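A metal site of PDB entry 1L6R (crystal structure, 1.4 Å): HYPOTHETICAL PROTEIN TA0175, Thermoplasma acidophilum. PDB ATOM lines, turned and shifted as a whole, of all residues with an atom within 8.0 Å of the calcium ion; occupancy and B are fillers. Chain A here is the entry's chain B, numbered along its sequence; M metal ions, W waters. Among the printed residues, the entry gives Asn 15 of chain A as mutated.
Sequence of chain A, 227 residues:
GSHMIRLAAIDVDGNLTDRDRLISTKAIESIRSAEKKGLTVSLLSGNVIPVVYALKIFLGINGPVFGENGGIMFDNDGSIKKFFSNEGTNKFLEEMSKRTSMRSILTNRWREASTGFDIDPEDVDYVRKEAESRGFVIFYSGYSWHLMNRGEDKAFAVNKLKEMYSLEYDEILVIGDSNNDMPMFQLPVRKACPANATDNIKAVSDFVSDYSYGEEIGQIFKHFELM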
ATOM      1  N   ILE A  10      31.551   3.678 -21.422  1.00  0.00           N
ATOM      2  CA  ILE A  10      30.699   2.717 -22.092  1.00  0.00           C
ATOM      3  C   ILE A  10      29.740   3.294 -23.121  1.00  0.00           C
ATOM      4  O   ILE A  10      28.964   4.215 -22.828  1.00  0.00           O
ATOM      5  CB  ILE A  10      29.846   1.940 -21.051  1.00  0.00           C
ATOM      6  CG1 ILE A  10      30.739   1.428 -19.928  1.00  0.00           C
ATOM      7  CG2 ILE A  10      29.109   0.807 -21.727  1.00  0.00           C
ATOM      8  CD1 ILE A  10      29.986   0.740 -18.787  1.00  0.00           C
ATOM      9  N   ASP A  11      29.818   2.767 -24.333  1.00  0.00           N
ATOM     10  CA  ASP A  11      28.908   3.197 -25.386  1.00  0.00           C
ATOM     11  C   ASP A  11      27.566   2.519 -25.082  1.00  0.00           C
ATOM     12  O   ASP A  11      27.511   1.319 -24.814  1.00  0.00           O
ATOM     13  CB  ASP A  11      29.429   2.760 -26.736  1.00  0.00           C
ATOM     14  CG  ASP A  11      28.392   2.889 -27.801  1.00  0.00           C
ATOM     15  OD1 ASP A  11      28.066   4.015 -28.245  1.00  0.00           O
ATOM     16  OD2 ASP A  11      27.845   1.852 -28.179  1.00  0.00           O
ATOM     17  N   VAL A  12      26.480   3.285 -25.134  1.00  0.00           N
ATOM     18  CA  VAL A  12      25.175   2.743 -24.803  1.00  0.00           C
ATOM     19  C   VAL A  12      24.563   1.747 -25.780  1.00  0.00           C
ATOM     20  O   VAL A  12      24.309   0.598 -25.430  1.00  0.00           O
ATOM     21  CB  VAL A  12      24.162   3.898 -24.568  1.00  0.00           C
ATOM     22  CG1 VAL A  12      22.776   3.322 -24.273  1.00  0.00           C
ATOM     23  CG2 VAL A  12      24.635   4.791 -23.431  1.00  0.00           C
ATOM     24  N   ASP A  13      24.359   2.189 -27.012  1.00  0.00           N
ATOM     25  CA  ASP A  13      23.697   1.375 -28.013  1.00  0.00           C
ATOM     26  C   ASP A  13      24.461   0.130 -28.412  1.00  0.00           C
ATOM     27  O   ASP A  13      25.549   0.213 -28.959  1.00  0.00           O
ATOM     28  CB  ASP A  13      23.418   2.213 -29.266  1.00  0.00           C
ATOM     29  CG  ASP A  13      22.520   1.503 -30.246  1.00  0.00           C
ATOM     30  OD1 ASP A  13      21.296   1.514 -30.031  1.00  0.00           O
ATOM     31  OD2 ASP A  13      23.035   0.902 -31.218  1.00  0.00           O
ATOM     32  N   GLY A  14      23.888  -1.038 -28.144  1.00  0.00           N
ATOM     33  CA  GLY A  14      24.552  -2.277 -28.495  1.00  0.00           C
ATOM     34  C   GLY A  14      25.364  -2.898 -27.381  1.00  0.00           C
ATOM     35  O   GLY A  14      25.840  -4.028 -27.515  1.00  0.00           O
ATOM     36  N   ASN A  15      25.528  -2.167 -26.280  1.00  0.00           N
ATOM     37  CA  ASN A  15      26.292  -2.661 -25.136  1.00  0.00           C
ATOM     38  C   ASN A  15      25.464  -2.686 -23.863  1.00  0.00           C
ATOM     39  O   ASN A  15      25.626  -3.565 -23.024  1.00  0.00           O
ATOM     40  CB  ASN A  15      27.550  -1.826 -24.942  1.00  0.00           C
ATOM     41  CG  ASN A  15      28.443  -1.875 -26.157  1.00  0.00           C
ATOM     42  OD1 ASN A  15      29.138  -2.858 -26.384  1.00  0.00           O
ATOM     43  ND2 ASN A  15      28.409  -0.815 -26.963  1.00  0.00           N
ATOM     44  N   LEU A  16      24.599  -1.694 -23.697  1.00  0.00           N
ATOM     45  CA  LEU A  16      23.730  -1.652 -22.534  1.00  0.00           C
ATOM     46  C   LEU A  16      22.290  -1.960 -22.946  1.00  0.00           C
ATOM     47  O   LEU A  16      21.389  -1.949 -22.110  1.00  0.00           O
ATOM     48  CB  LEU A  16      23.760  -0.276 -21.859  1.00  0.00           C
ATOM     49  CG  LEU A  16      25.119   0.179 -21.332  1.00  0.00           C
ATOM     50  CD1 LEU A  16      25.002   1.519 -20.609  1.00  0.00           C
ATOM     51  CD2 LEU A  16      25.673  -0.882 -20.378  1.00  0.00           C
ATOM     52  N   THR A  17      22.088  -2.217 -24.235  1.00  0.00           N
ATOM     53  CA  THR A  17      20.743  -2.498 -24.751  1.00  0.00           C
ATOM     54  C   THR A  17      20.581  -3.932 -25.262  1.00  0.00           C
ATOM     55  O   THR A  17      21.550  -4.569 -25.653  1.00  0.00           O
ATOM     56  CB  THR A  17      20.402  -1.524 -25.892  1.00  0.00           C
ATOM     57  OG1 THR A  17      21.382  -1.618 -26.933  1.00  0.00           O
ATOM     58  CG2 THR A  17      20.365  -0.105 -25.365  1.00  0.00           C
ATOM     59  N   LEU A  44      28.333   7.067 -23.134  1.00  0.00           N
ATOM     60  CA  LEU A  44      28.418   7.840 -24.360  1.00  0.00           C
ATOM     61  C   LEU A  44      27.438   7.293 -25.388  1.00  0.00           C
ATOM     62  O   LEU A  44      27.277   6.080 -25.514  1.00  0.00           O
ATOM     63  CB  LEU A  44      29.819   7.766 -24.961  1.00  0.00           C
ATOM     64  CG  LEU A  44      30.983   8.183 -24.061  1.00  0.00           C
ATOM     65  CD1 LEU A  44      31.478   7.002 -23.234  1.00  0.00           C
ATOM     66  CD2 LEU A  44      32.095   8.738 -24.921  1.00  0.00           C
ATOM     67  N   SER A  45      26.764   8.182 -26.108  1.00  0.00           N
ATOM     68  CA  SER A  45      25.860   7.730 -27.166  1.00  0.00           C
ATOM     69  C   SER A  45      25.623   8.844 -28.149  1.00  0.00           C
ATOM     70  O   SER A  45      26.179   9.935 -28.009  1.00  0.00           O
ATOM     71  CB  SER A  45      24.510   7.263 -26.595  1.00  0.00           C
ATOM     72  OG  SER A  45      23.673   8.358 -26.261  1.00  0.00           O
ATOM     73  N   SER A 141      23.841   5.441 -36.570  1.00  0.00           N
ATOM     74  CA  SER A 141      24.025   4.783 -35.287  1.00  0.00           C
ATOM     75  C   SER A 141      22.890   5.116 -34.349  1.00  0.00           C
ATOM     76  O   SER A 141      22.435   6.254 -34.282  1.00  0.00           O
ATOM     77  CB  SER A 141      25.358   5.168 -34.656  1.00  0.00           C
ATOM     78  OG  SER A 141      25.563   4.386 -33.485  1.00  0.00           O
ATOM     79  N   GLY A 142      22.405   4.104 -33.640  1.00  0.00           N
ATOM     80  CA  GLY A 142      21.344   4.324 -32.692  1.00  0.00           C
ATOM     81  C   GLY A 142      19.970   4.470 -33.292  1.00  0.00           C
ATOM     82  O   GLY A 142      19.359   3.489 -33.721  1.00  0.00           O
ATOM     83  N   LYS A 154      33.858   9.598 -30.083  1.00  0.00           N
ATOM     84  CA  LYS A 154      34.070   9.059 -28.763  1.00  0.00           C
ATOM     85  C   LYS A 154      35.506   9.100 -28.266  1.00  0.00           C
ATOM     86  O   LYS A 154      35.742   9.083 -27.062  1.00  0.00           O
ATOM     87  CB  LYS A 154      33.483   7.650 -28.665  1.00  0.00           C
ATOM     88  CG  LYS A 154      31.967   7.655 -28.797  1.00  0.00           C
ATOM     89  CD  LYS A 154      31.379   6.313 -28.359  1.00  0.00           C
ATOM     90  CE  LYS A 154      29.884   6.251 -28.589  1.00  0.00           C
ATOM     91  NZ  LYS A 154      29.547   5.760 -29.968  1.00  0.00           N
ATOM     92  N   ILE A 175      34.245   0.143 -23.458  1.00  0.00           N
ATOM     93  CA  ILE A 175      33.362  -0.948 -23.866  1.00  0.00           C
ATOM     94  C   ILE A 175      32.524  -0.435 -25.044  1.00  0.00           C
ATOM     95  O   ILE A 175      31.822   0.579 -24.938  1.00  0.00           O
ATOM     96  CB  ILE A 175      32.440  -1.398 -22.710  1.00  0.00           C
ATOM     97  CG1 ILE A 175      33.306  -1.905 -21.545  1.00  0.00           C
ATOM     98  CG2 ILE A 175      31.507  -2.505 -23.195  1.00  0.00           C
ATOM     99  CD1 ILE A 175      32.510  -2.308 -20.320  1.00  0.00           C
ATOM    100  N   GLY A 176      32.613  -1.141 -26.163  1.00  0.00           N
ATOM    101  CA  GLY A 176      31.906  -0.758 -27.380  1.00  0.00           C
ATOM    102  C   GLY A 176      31.669  -1.969 -28.247  1.00  0.00           C
ATOM    103  O   GLY A 176      32.192  -3.043 -27.956  1.00  0.00           O
ATOM    104  N   ASP A 177      30.935  -1.789 -29.348  1.00  0.00           N
ATOM    105  CA  ASP A 177      30.597  -2.927 -30.191  1.00  0.00           C
ATOM    106  C   ASP A 177      30.463  -2.643 -31.688  1.00  0.00           C
ATOM    107  O   ASP A 177      30.531  -3.564 -32.484  1.00  0.00           O
ATOM    108  CB  ASP A 177      29.271  -3.515 -29.721  1.00  0.00           C
ATOM    109  CG  ASP A 177      28.086  -2.661 -30.150  1.00  0.00           C
ATOM    110  OD1 ASP A 177      28.146  -1.442 -29.918  1.00  0.00           O
ATOM    111  OD2 ASP A 177      27.111  -3.181 -30.714  1.00  0.00           O
ATOM    112  N   SER A 178      30.252  -1.387 -32.064  1.00  0.00           N
ATOM    113  CA  SER A 178      30.044  -1.063 -33.479  1.00  0.00           C
ATOM    114  C   SER A 178      31.154  -0.205 -34.084  1.00  0.00           C
ATOM    115  O   SER A 178      32.053   0.259 -33.380  1.00  0.00           O
ATOM    116  CB  SER A 178      28.685  -0.389 -33.639  1.00  0.00           C
ATOM    117  OG  SER A 178      28.530   0.700 -32.756  1.00  0.00           O
ATOM    118  N   ASN A 179      31.079   0.019 -35.391  1.00  0.00           N
ATOM    119  CA  ASN A 179      32.123   0.789 -36.063  1.00  0.00           C
ATOM    120  C   ASN A 179      32.331   2.189 -35.501  1.00  0.00           C
ATOM    121  O   ASN A 179      33.463   2.666 -35.447  1.00  0.00           O
ATOM    122  CB  ASN A 179      31.875   0.869 -37.567  1.00  0.00           C
ATOM    123  CG  ASN A 179      32.953   1.679 -38.278  1.00  0.00           C
ATOM    124  OD1 ASN A 179      32.742   2.841 -38.621  1.00  0.00           O
ATOM    125  ND2 ASN A 179      34.121   1.069 -38.474  1.00  0.00           N
ATOM    126  N   ASN A 180      31.255   2.836 -35.083  1.00  0.00           N
ATOM    127  CA  ASN A 180      31.395   4.185 -34.544  1.00  0.00           C
ATOM    128  C   ASN A 180      31.973   4.171 -33.124  1.00  0.00           C
ATOM    129  O   ASN A 180      32.147   5.220 -32.503  1.00  0.00           O
ATOM    130  CB  ASN A 180      30.059   4.918 -34.599  1.00  0.00           C
ATOM    131  CG  ASN A 180      28.981   4.203 -33.831  1.00  0.00           C
ATOM    132  OD1 ASN A 180      28.586   3.084 -34.171  1.00  0.00           O
ATOM    133  ND2 ASN A 180      28.484   4.849 -32.791  1.00  0.00           N
ATOM    134  N   ASP A 181      32.271   2.974 -32.611  1.00  0.00           N
ATOM    135  CA  ASP A 181      32.886   2.860 -31.295  1.00  0.00           C
ATOM    136  C   ASP A 181      34.391   2.616 -31.447  1.00  0.00           C
ATOM    137  O   ASP A 181      35.155   2.783 -30.504  1.00  0.00           O
ATOM    138  CB  ASP A 181      32.281   1.687 -30.504  1.00  0.00           C
ATOM    139  CG  ASP A 181      30.821   1.886 -30.206  1.00  0.00           C
ATOM    140  OD1 ASP A 181      30.397   3.034 -29.963  1.00  0.00           O
ATOM    141  OD2 ASP A 181      30.084   0.882 -30.193  1.00  0.00           O
ATOM    142  N   MET A 182      34.796   2.247 -32.663  1.00  0.00           N
ATOM    143  CA  MET A 182      36.216   1.983 -32.932  1.00  0.00           C
ATOM    144  C   MET A 182      37.147   3.135 -32.531  1.00  0.00           C
ATOM    145  O   MET A 182      38.293   2.899 -32.126  1.00  0.00           O
ATOM    146  CB  MET A 182      36.401   1.615 -34.413  1.00  0.00           C
ATOM    147  CG  MET A 182      37.839   1.300 -34.796  1.00  0.00           C
ATOM    148  SD  MET A 182      38.593  -0.093 -33.882  1.00  0.00           S
ATOM    149  CE  MET A 182      38.053  -1.500 -34.877  1.00  0.00           C
ATOM    150  N   MET A 184      37.335   4.762 -29.902  1.00  0.00           N
ATOM    151  CA  MET A 184      37.779   4.505 -28.536  1.00  0.00           C
ATOM    152  C   MET A 184      38.832   3.408 -28.490  1.00  0.00           C
ATOM    153  O   MET A 184      39.768   3.462 -27.688  1.00  0.00           O
ATOM    154  CB  MET A 184      36.605   4.067 -27.649  1.00  0.00           C
ATOM    155  CG  MET A 184      35.497   5.089 -27.488  1.00  0.00           C
ATOM    156  SD  MET A 184      34.395   4.651 -26.120  1.00  0.00           S
ATOM    157  CE  MET A 184      33.599   3.173 -26.752  1.00  0.00           C
ATOM    158  N   PRO A 194      31.167  -6.937 -26.280  1.00  0.00           N
ATOM    159  CA  PRO A 194      30.221  -8.051 -26.157  1.00  0.00           C
ATOM    160  C   PRO A 194      30.558  -9.103 -27.204  1.00  0.00           C
ATOM    161  O   PRO A 194      31.320  -8.832 -28.143  1.00  0.00           O
ATOM    162  CB  PRO A 194      28.862  -7.387 -26.404  1.00  0.00           C
ATOM    163  CG  PRO A 194      29.204  -6.222 -27.304  1.00  0.00           C
ATOM    164  CD  PRO A 194      30.468  -5.698 -26.674  1.00  0.00           C
HETATM  165 CA    CA M   1      27.535   0.802 -30.320  1.00  0.00          CA
HETATM  166  O   HOH W   1      25.530   0.672 -31.932  1.00  0.00           O
HETATM  167  O   HOH W   2      27.298   3.226 -30.786  1.00  0.00           O
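The calcium ion is bound by OD1 of Asp 177 (2.4 Å), OD2 of Asp 11 (2.4 Å), O of Asp 13 (2.5 Å), water W2 (2.5 Å), OD2 of Asp 181 (2.6 Å), water W1 (2.6 Å) and OG of Ser 178 (2.6 Å).
The calcium ion has seven donor atoms within binding distance.
Water W2 lies within hydrogen-bond range of OD1 of Asp 11, ND2 of Asn 180, OD1 of Asp 181, OG of Ser 141 and NZ of Lys 154.
Asn 15 touches the calcium ion.
Six residues have an atom within 4 Å of the calcium ion: Asp 11, Asp 13, Asn 15, Asp 177, Ser 178 and Asp 181.
The side-chain carboxylate (OD1) of Asp 177 lies close to the side-chain amide nitrogen (ND2) of Asn 15 (3.0 Å).
The backbone carbonyl oxygen of Asp 11 sits close to the side-chain amide nitrogen of Asn 15, at 3.2 Å.
NZ of Lys 154 is in salt-bridge range of OD1 of Asp 11 (2.9 Å).
The backbone NH of Asp 11 lies within hydrogen-bond range of the backbone carbonyl oxygen of Ile 175, at 3.0 Å.
OD1 of Asp 181 lies within salt-bridge range of NZ of Lys 154, at 2.9 Å.
The side-chain hydroxyl (OG) of Ser 178 sits close to the side-chain amide oxygen (OD1) of Asn 180 (2.8 Å).
The side-chain amide oxygen of Asn 15 lies close to the backbone carbonyl oxygen of Gly 176, at 3.4 Å.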
